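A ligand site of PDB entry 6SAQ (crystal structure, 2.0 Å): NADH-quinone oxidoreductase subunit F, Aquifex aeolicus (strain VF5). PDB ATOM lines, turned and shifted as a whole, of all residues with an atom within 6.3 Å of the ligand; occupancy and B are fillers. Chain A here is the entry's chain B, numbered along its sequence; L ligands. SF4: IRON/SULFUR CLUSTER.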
ATOM      1  N   ILE A 181     -10.684  11.712  34.525  1.00  0.00           N
ATOM      2  CA  ILE A 181     -11.652  11.099  33.607  1.00  0.00           C
ATOM      3  C   ILE A 181     -13.032  10.926  34.254  1.00  0.00           C
ATOM      4  O   ILE A 181     -14.012  10.856  33.529  1.00  0.00           O
ATOM      5  CB  ILE A 181     -11.096   9.790  32.979  1.00  0.00           C
ATOM      6  CG1 ILE A 181     -11.889   9.363  31.698  1.00  0.00           C
ATOM      7  CG2 ILE A 181     -11.002   8.646  34.017  1.00  0.00           C
ATOM      8  CD1 ILE A 181     -11.989  10.401  30.632  1.00  0.00           C
ATOM      9  N   HIS A 198     -14.441   4.274  33.718  1.00  0.00           N
ATOM     10  CA  HIS A 198     -14.246   4.076  32.286  1.00  0.00           C
ATOM     11  C   HIS A 198     -15.426   4.660  31.480  1.00  0.00           C
ATOM     12  O   HIS A 198     -16.543   4.152  31.616  1.00  0.00           O
ATOM     13  CB  HIS A 198     -14.055   2.582  31.944  1.00  0.00           C
ATOM     14  CG  HIS A 198     -12.757   2.000  32.413  1.00  0.00           C
ATOM     15  ND1 HIS A 198     -12.689   0.718  32.909  1.00  0.00           N
ATOM     16  CD2 HIS A 198     -11.523   2.539  32.430  1.00  0.00           C
ATOM     17  CE1 HIS A 198     -11.417   0.517  33.220  1.00  0.00           C
ATOM     18  NE2 HIS A 198     -10.682   1.585  32.961  1.00  0.00           N
ATOM     19  N   PRO A 199     -15.202   5.658  30.607  1.00  0.00           N
ATOM     20  CA  PRO A 199     -16.295   6.159  29.766  1.00  0.00           C
ATOM     21  C   PRO A 199     -16.975   5.052  28.948  1.00  0.00           C
ATOM     22  O   PRO A 199     -16.380   4.004  28.618  1.00  0.00           O
ATOM     23  CB  PRO A 199     -15.598   7.162  28.852  1.00  0.00           C
ATOM     24  CG  PRO A 199     -14.461   7.665  29.659  1.00  0.00           C
ATOM     25  CD  PRO A 199     -13.955   6.424  30.345  1.00  0.00           C
ATOM     26  N   ARG A 200     -18.233   5.285  28.627  1.00  0.00           N
ATOM     27  CA  ARG A 200     -19.052   4.375  27.830  1.00  0.00           C
ATOM     28  C   ARG A 200     -19.141   4.980  26.437  1.00  0.00           C
ATOM     29  O   ARG A 200     -19.114   6.192  26.285  1.00  0.00           O
ATOM     30  CB  ARG A 200     -20.482   4.300  28.395  1.00  0.00           C
ATOM     31  CG  ARG A 200     -20.627   3.822  29.833  1.00  0.00           C
ATOM     32  CD  ARG A 200     -22.062   4.029  30.277  1.00  0.00           C
ATOM     33  NE  ARG A 200     -22.319   3.464  31.604  1.00  0.00           N
ATOM     34  CZ  ARG A 200     -23.479   3.523  32.251  1.00  0.00           C
ATOM     35  NH1 ARG A 200     -24.520   4.141  31.716  1.00  0.00           N
ATOM     36  NH2 ARG A 200     -23.605   2.938  33.440  1.00  0.00           N
ATOM     37  N   GLU A 345      -3.732  10.955  32.913  1.00  0.00           N
ATOM     38  CA  GLU A 345      -5.196  10.842  33.028  1.00  0.00           C
ATOM     39  C   GLU A 345      -5.922   9.906  32.050  1.00  0.00           C
ATOM     40  O   GLU A 345      -7.079   9.572  32.322  1.00  0.00           O
ATOM     41  CB  GLU A 345      -5.839  12.247  32.973  1.00  0.00           C
ATOM     42  CG  GLU A 345      -5.324  13.161  34.093  1.00  0.00           C
ATOM     43  CD  GLU A 345      -5.511  12.766  35.550  1.00  0.00           C
ATOM     44  OE1 GLU A 345      -6.348  11.878  35.852  1.00  0.00           O
ATOM     45  OE2 GLU A 345      -4.827  13.365  36.417  1.00  0.00           O
ATOM     46  N   THR A 346      -5.296   9.489  30.939  1.00  0.00           N
ATOM     47  CA  THR A 346      -5.955   8.522  30.054  1.00  0.00           C
ATOM     48  C   THR A 346      -6.396   7.276  30.859  1.00  0.00           C
ATOM     49  O   THR A 346      -5.618   6.775  31.672  1.00  0.00           O
ATOM     50  CB  THR A 346      -5.077   8.126  28.850  1.00  0.00           C
ATOM     51  OG1 THR A 346      -5.735   7.059  28.149  1.00  0.00           O
ATOM     52  CG2 THR A 346      -3.649   7.685  29.253  1.00  0.00           C
ATOM     53  N   CYS A 347      -7.639   6.798  30.670  1.00  0.00           N
ATOM     54  CA  CYS A 347      -8.122   5.605  31.398  1.00  0.00           C
ATOM     55  C   CYS A 347      -7.540   4.315  30.799  1.00  0.00           C
ATOM     56  O   CYS A 347      -7.582   3.275  31.432  1.00  0.00           O
ATOM     57  CB  CYS A 347      -9.652   5.551  31.485  1.00  0.00           C
ATOM     58  SG  CYS A 347     -10.477   5.025  29.968  1.00  0.00           S
ATOM     59  N   GLY A 348      -7.004   4.401  29.588  1.00  0.00           N
ATOM     60  CA  GLY A 348      -6.343   3.289  28.915  1.00  0.00           C
ATOM     61  C   GLY A 348      -7.223   2.298  28.182  1.00  0.00           C
ATOM     62  O   GLY A 348      -6.701   1.312  27.661  1.00  0.00           O
ATOM     63  N   GLN A 349      -8.544   2.538  28.096  1.00  0.00           N
ATOM     64  CA  GLN A 349      -9.461   1.606  27.380  1.00  0.00           C
ATOM     65  C   GLN A 349      -9.170   1.504  25.863  1.00  0.00           C
ATOM     66  O   GLN A 349      -9.371   0.454  25.266  1.00  0.00           O
ATOM     67  CB  GLN A 349     -10.913   2.113  27.495  1.00  0.00           C
ATOM     68  CG  GLN A 349     -11.683   1.609  28.662  1.00  0.00           C
ATOM     69  CD  GLN A 349     -13.143   1.965  28.445  1.00  0.00           C
ATOM     70  OE1 GLN A 349     -13.953   1.099  28.124  1.00  0.00           O
ATOM     71  NE2 GLN A 349     -13.520   3.252  28.580  1.00  0.00           N
ATOM     72  N   CYS A 350      -8.838   2.633  25.235  1.00  0.00           N
ATOM     73  CA  CYS A 350      -8.633   2.764  23.797  1.00  0.00           C
ATOM     74  C   CYS A 350      -7.104   2.756  23.540  1.00  0.00           C
ATOM     75  O   CYS A 350      -6.373   3.454  24.229  1.00  0.00           O
ATOM     76  CB  CYS A 350      -9.308   4.034  23.273  1.00  0.00           C
ATOM     77  SG  CYS A 350     -10.995   4.307  23.919  1.00  0.00           S
ATOM     78  N   THR A 351      -6.637   1.916  22.610  1.00  0.00           N
ATOM     79  CA  THR A 351      -5.192   1.743  22.347  1.00  0.00           C
ATOM     80  C   THR A 351      -4.505   3.031  21.866  1.00  0.00           C
ATOM     81  O   THR A 351      -3.523   3.397  22.520  1.00  0.00           O
ATOM     82  CB  THR A 351      -4.923   0.511  21.433  1.00  0.00           C
ATOM     83  OG1 THR A 351      -5.249  -0.657  22.204  1.00  0.00           O
ATOM     84  CG2 THR A 351      -3.463   0.415  20.995  1.00  0.00           C
ATOM     85  N   CYS A 353      -5.262   6.152  22.330  1.00  0.00           N
ATOM     86  CA  CYS A 353      -5.258   7.112  23.457  1.00  0.00           C
ATOM     87  C   CYS A 353      -4.251   6.617  24.541  1.00  0.00           C
ATOM     88  O   CYS A 353      -3.409   7.397  24.970  1.00  0.00           O
ATOM     89  CB  CYS A 353      -6.661   7.309  24.037  1.00  0.00           C
ATOM     90  SG  CYS A 353      -6.729   8.429  25.472  1.00  0.00           S
ATOM     91  N   ARG A 354      -4.354   5.327  24.966  1.00  0.00           N
ATOM     92  CA  ARG A 354      -3.457   4.727  25.956  1.00  0.00           C
ATOM     93  C   ARG A 354      -1.972   4.912  25.584  1.00  0.00           C
ATOM     94  O   ARG A 354      -1.194   5.465  26.372  1.00  0.00           O
ATOM     95  CB  ARG A 354      -3.756   3.236  26.118  1.00  0.00           C
ATOM     96  CG  ARG A 354      -2.852   2.483  27.130  1.00  0.00           C
ATOM     97  CD  ARG A 354      -3.342   1.034  27.339  1.00  0.00           C
ATOM     98  NE  ARG A 354      -2.993   0.209  26.187  1.00  0.00           N
ATOM     99  CZ  ARG A 354      -3.841  -0.238  25.279  1.00  0.00           C
ATOM    100  NH1 ARG A 354      -5.152  -0.014  25.413  1.00  0.00           N
ATOM    101  NH2 ARG A 354      -3.400  -0.946  24.247  1.00  0.00           N
ATOM    102  N   CYS A 357      -1.051   9.023  24.439  1.00  0.00           N
ATOM    103  CA  CYS A 357      -0.865   9.996  25.541  1.00  0.00           C
ATOM    104  C   CYS A 357       0.482   9.755  26.206  1.00  0.00           C
ATOM    105  O   CYS A 357       1.178  10.709  26.557  1.00  0.00           O
ATOM    106  CB  CYS A 357      -2.005   9.919  26.558  1.00  0.00           C
ATOM    107  SG  CYS A 357      -3.578  10.605  25.966  1.00  0.00           S
ATOM    108  N   ILE A 387      -3.694  10.237  18.396  1.00  0.00           N
ATOM    109  CA  ILE A 387      -4.209   9.826  19.722  1.00  0.00           C
ATOM    110  C   ILE A 387      -5.713   9.538  19.617  1.00  0.00           C
ATOM    111  O   ILE A 387      -6.215   8.591  20.225  1.00  0.00           O
ATOM    112  CB  ILE A 387      -3.901  10.902  20.804  1.00  0.00           C
ATOM    113  CG1 ILE A 387      -2.387  11.130  20.964  1.00  0.00           C
ATOM    114  CG2 ILE A 387      -4.569  10.531  22.172  1.00  0.00           C
ATOM    115  CD1 ILE A 387      -1.969  12.416  21.783  1.00  0.00           C
ATOM    116  N   THR A 390     -10.269   5.749  17.060  1.00  0.00           N
ATOM    117  CA  THR A 390     -11.039   4.727  17.842  1.00  0.00           C
ATOM    118  C   THR A 390     -11.436   5.228  19.250  1.00  0.00           C
ATOM    119  O   THR A 390     -12.121   4.485  19.968  1.00  0.00           O
ATOM    120  CB  THR A 390     -10.322   3.338  17.902  1.00  0.00           C
ATOM    121  OG1 THR A 390      -9.334   3.357  18.943  1.00  0.00           O
ATOM    122  CG2 THR A 390      -9.663   2.926  16.570  1.00  0.00           C
ATOM    123  N   SER A 391     -11.021   6.453  19.664  1.00  0.00           N
ATOM    124  CA  SER A 391     -11.352   7.006  20.998  1.00  0.00           C
ATOM    125  C   SER A 391     -12.856   7.030  21.252  1.00  0.00           C
ATOM    126  O   SER A 391     -13.632   7.352  20.353  1.00  0.00           O
ATOM    127  CB  SER A 391     -10.766   8.411  21.189  1.00  0.00           C
ATOM    128  OG  SER A 391     -11.313   9.331  20.280  1.00  0.00           O
ATOM    129  N   ILE A 392     -13.266   6.679  22.454  1.00  0.00           N
ATOM    130  CA  ILE A 392     -14.705   6.682  22.735  1.00  0.00           C
ATOM    131  C   ILE A 392     -15.091   7.837  23.661  1.00  0.00           C
ATOM    132  O   ILE A 392     -16.259   7.954  24.031  1.00  0.00           O
ATOM    133  CB  ILE A 392     -15.263   5.303  23.188  1.00  0.00           C
ATOM    134  CG1 ILE A 392     -14.698   4.845  24.535  1.00  0.00           C
ATOM    135  CG2 ILE A 392     -15.060   4.250  22.076  1.00  0.00           C
ATOM    136  CD1 ILE A 392     -15.277   3.474  25.068  1.00  0.00           C
ATOM    137  N   CYS A 393     -14.150   8.726  24.000  1.00  0.00           N
ATOM    138  CA  CYS A 393     -14.505   9.887  24.800  1.00  0.00           C
ATOM    139  C   CYS A 393     -13.701  11.132  24.359  1.00  0.00           C
ATOM    140  O   CYS A 393     -12.800  11.017  23.529  1.00  0.00           O
ATOM    141  CB  CYS A 393     -14.447   9.621  26.306  1.00  0.00           C
ATOM    142  SG  CYS A 393     -12.888  10.102  27.098  1.00  0.00           S
ATOM    143  N   GLY A 394     -14.061  12.295  24.902  1.00  0.00           N
ATOM    144  CA  GLY A 394     -13.447  13.573  24.576  1.00  0.00           C
ATOM    145  C   GLY A 394     -11.976  13.717  24.941  1.00  0.00           C
ATOM    146  O   GLY A 394     -11.286  14.523  24.330  1.00  0.00           O
ATOM    147  N   LEU A 395     -11.477  12.933  25.914  1.00  0.00           N
ATOM    148  CA  LEU A 395     -10.055  13.007  26.287  1.00  0.00           C
ATOM    149  C   LEU A 395      -9.120  12.618  25.098  1.00  0.00           C
ATOM    150  O   LEU A 395      -8.222  13.390  24.759  1.00  0.00           O
ATOM    151  CB  LEU A 395      -9.744  12.190  27.547  1.00  0.00           C
ATOM    152  CG  LEU A 395      -8.357  12.418  28.213  1.00  0.00           C
ATOM    153  CD1 LEU A 395      -8.393  12.051  29.669  1.00  0.00           C
ATOM    154  CD2 LEU A 395      -7.214  11.590  27.501  1.00  0.00           C
ATOM    155  N   GLY A 396      -9.367  11.454  24.492  1.00  0.00           N
ATOM    156  CA  GLY A 396      -8.572  10.977  23.359  1.00  0.00           C
ATOM    157  C   GLY A 396      -8.695  11.901  22.159  1.00  0.00           C
ATOM    158  O   GLY A 396      -7.718  12.109  21.440  1.00  0.00           O
ATOM    159  N   ALA A 397      -9.889  12.518  21.990  1.00  0.00           N
ATOM    160  CA  ALA A 397     -10.146  13.463  20.906  1.00  0.00           C
ATOM    161  C   ALA A 397      -9.369  14.769  21.038  1.00  0.00           C
ATOM    162  O   ALA A 397      -9.094  15.393  20.023  1.00  0.00           O
ATOM    163  CB  ALA A 397     -11.641  13.761  20.789  1.00  0.00           C
HETATM  164 FE1  SF4 L   1     -10.214   6.304  28.149  1.00  0.00          FE
HETATM  165 FE2  SF4 L   1      -8.799   7.801  26.310  1.00  0.00          FE
HETATM  166 FE3  SF4 L   1     -11.466   8.308  26.755  1.00  0.00          FE
HETATM  167 FE4  SF4 L   1     -10.637   5.999  25.443  1.00  0.00          FE
HETATM  168  S1  SF4 L   1     -10.413   8.151  24.712  1.00  0.00           S
HETATM  169  S2  SF4 L   1     -12.260   6.168  27.061  1.00  0.00           S
HETATM  170  S3  SF4 L   1      -8.692   5.551  26.605  1.00  0.00           S
HETATM  171  S4  SF4 L   1      -9.729   8.543  28.273  1.00  0.00           S
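A sulfur (S3) of the ligand lies close to the backbone NH (N) of Gln 349.
The side-chain amide nitrogen (NE2) of Gln 349 lies close to a sulfur (S2) of the ligand, at 3.5 Å.
An iron atom (FE3) of the ligand is bound by the side-chain sulfur (SG) of Cys 393 (2.3 Å).
The backbone NH of Cys 350 lies close to a sulfur (S3) of the ligand, 3.2 Å away.
S3 of the ligand lies close to N of Gly 348 (3.6 Å).
OG1 of Thr 346 lies close to S3 of the ligand (3.7 Å).
SG of Cys 350 is bound to FE4 of the ligand, 2.3 Å away.
SG of Cys 347 binds FE1 of the ligand (2.2 Å).
The backbone NH (N) of Cys 347 sits close to a sulfur (S4) of the ligand.
The backbone NH (N) of Gly 396 lies close to a sulfur (S1) of the ligand (3.5 Å).
FE2 of the ligand is bound by SG of Cys 353.
N of Gly 348 lies close to OG1 of Thr 346, at 3.3 Å.
The backbone carbonyl oxygen (O) of Ile 387 is in hydrogen-bond range of the backbone NH (N) of Cys 353 (3.4 Å).
The backbone NH (N) of Gln 349 lies close to the side-chain sulfur (SG) of Cys 347.
The side-chain sulfur of Cys 393 lies close to the backbone NH of Leu 395.
O of Gly 348 lies within hydrogen-bond range of NH1 of Arg 354 (3.0 Å).
The backbone NH (N) of Ile 392 lies close to the side-chain sulfur (SG) of Cys 350, at 3.6 Å.
The backbone carbonyl oxygen (O) of Pro 199 is in hydrogen-bond range of the side-chain amide nitrogen (NE2) of Gln 349 (3.0 Å).
SG of Cys 357 lies close to O of Cys 353, at 3.4 Å.
Merely in contact with the ligand: Ser 391 (3.6 Å), Pro 199 (3.7 Å), Leu 395 (3.7 Å), Ile 392 (3.8 Å) and Ile 181 (3.8 Å).
Hydrophobic or aromatic side chains within 4 Å of the ligand: Ile 181, Pro 199, Ile 392 and Leu 395.
Of the 23 residues printed, 13 come within 4 Å of the ligand.
Along chain A the residues within 4 Å of the ligand span positions 181 to 396.
The nearest printed residue that does not touch the ligand is Arg 354 (4.6 Å).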
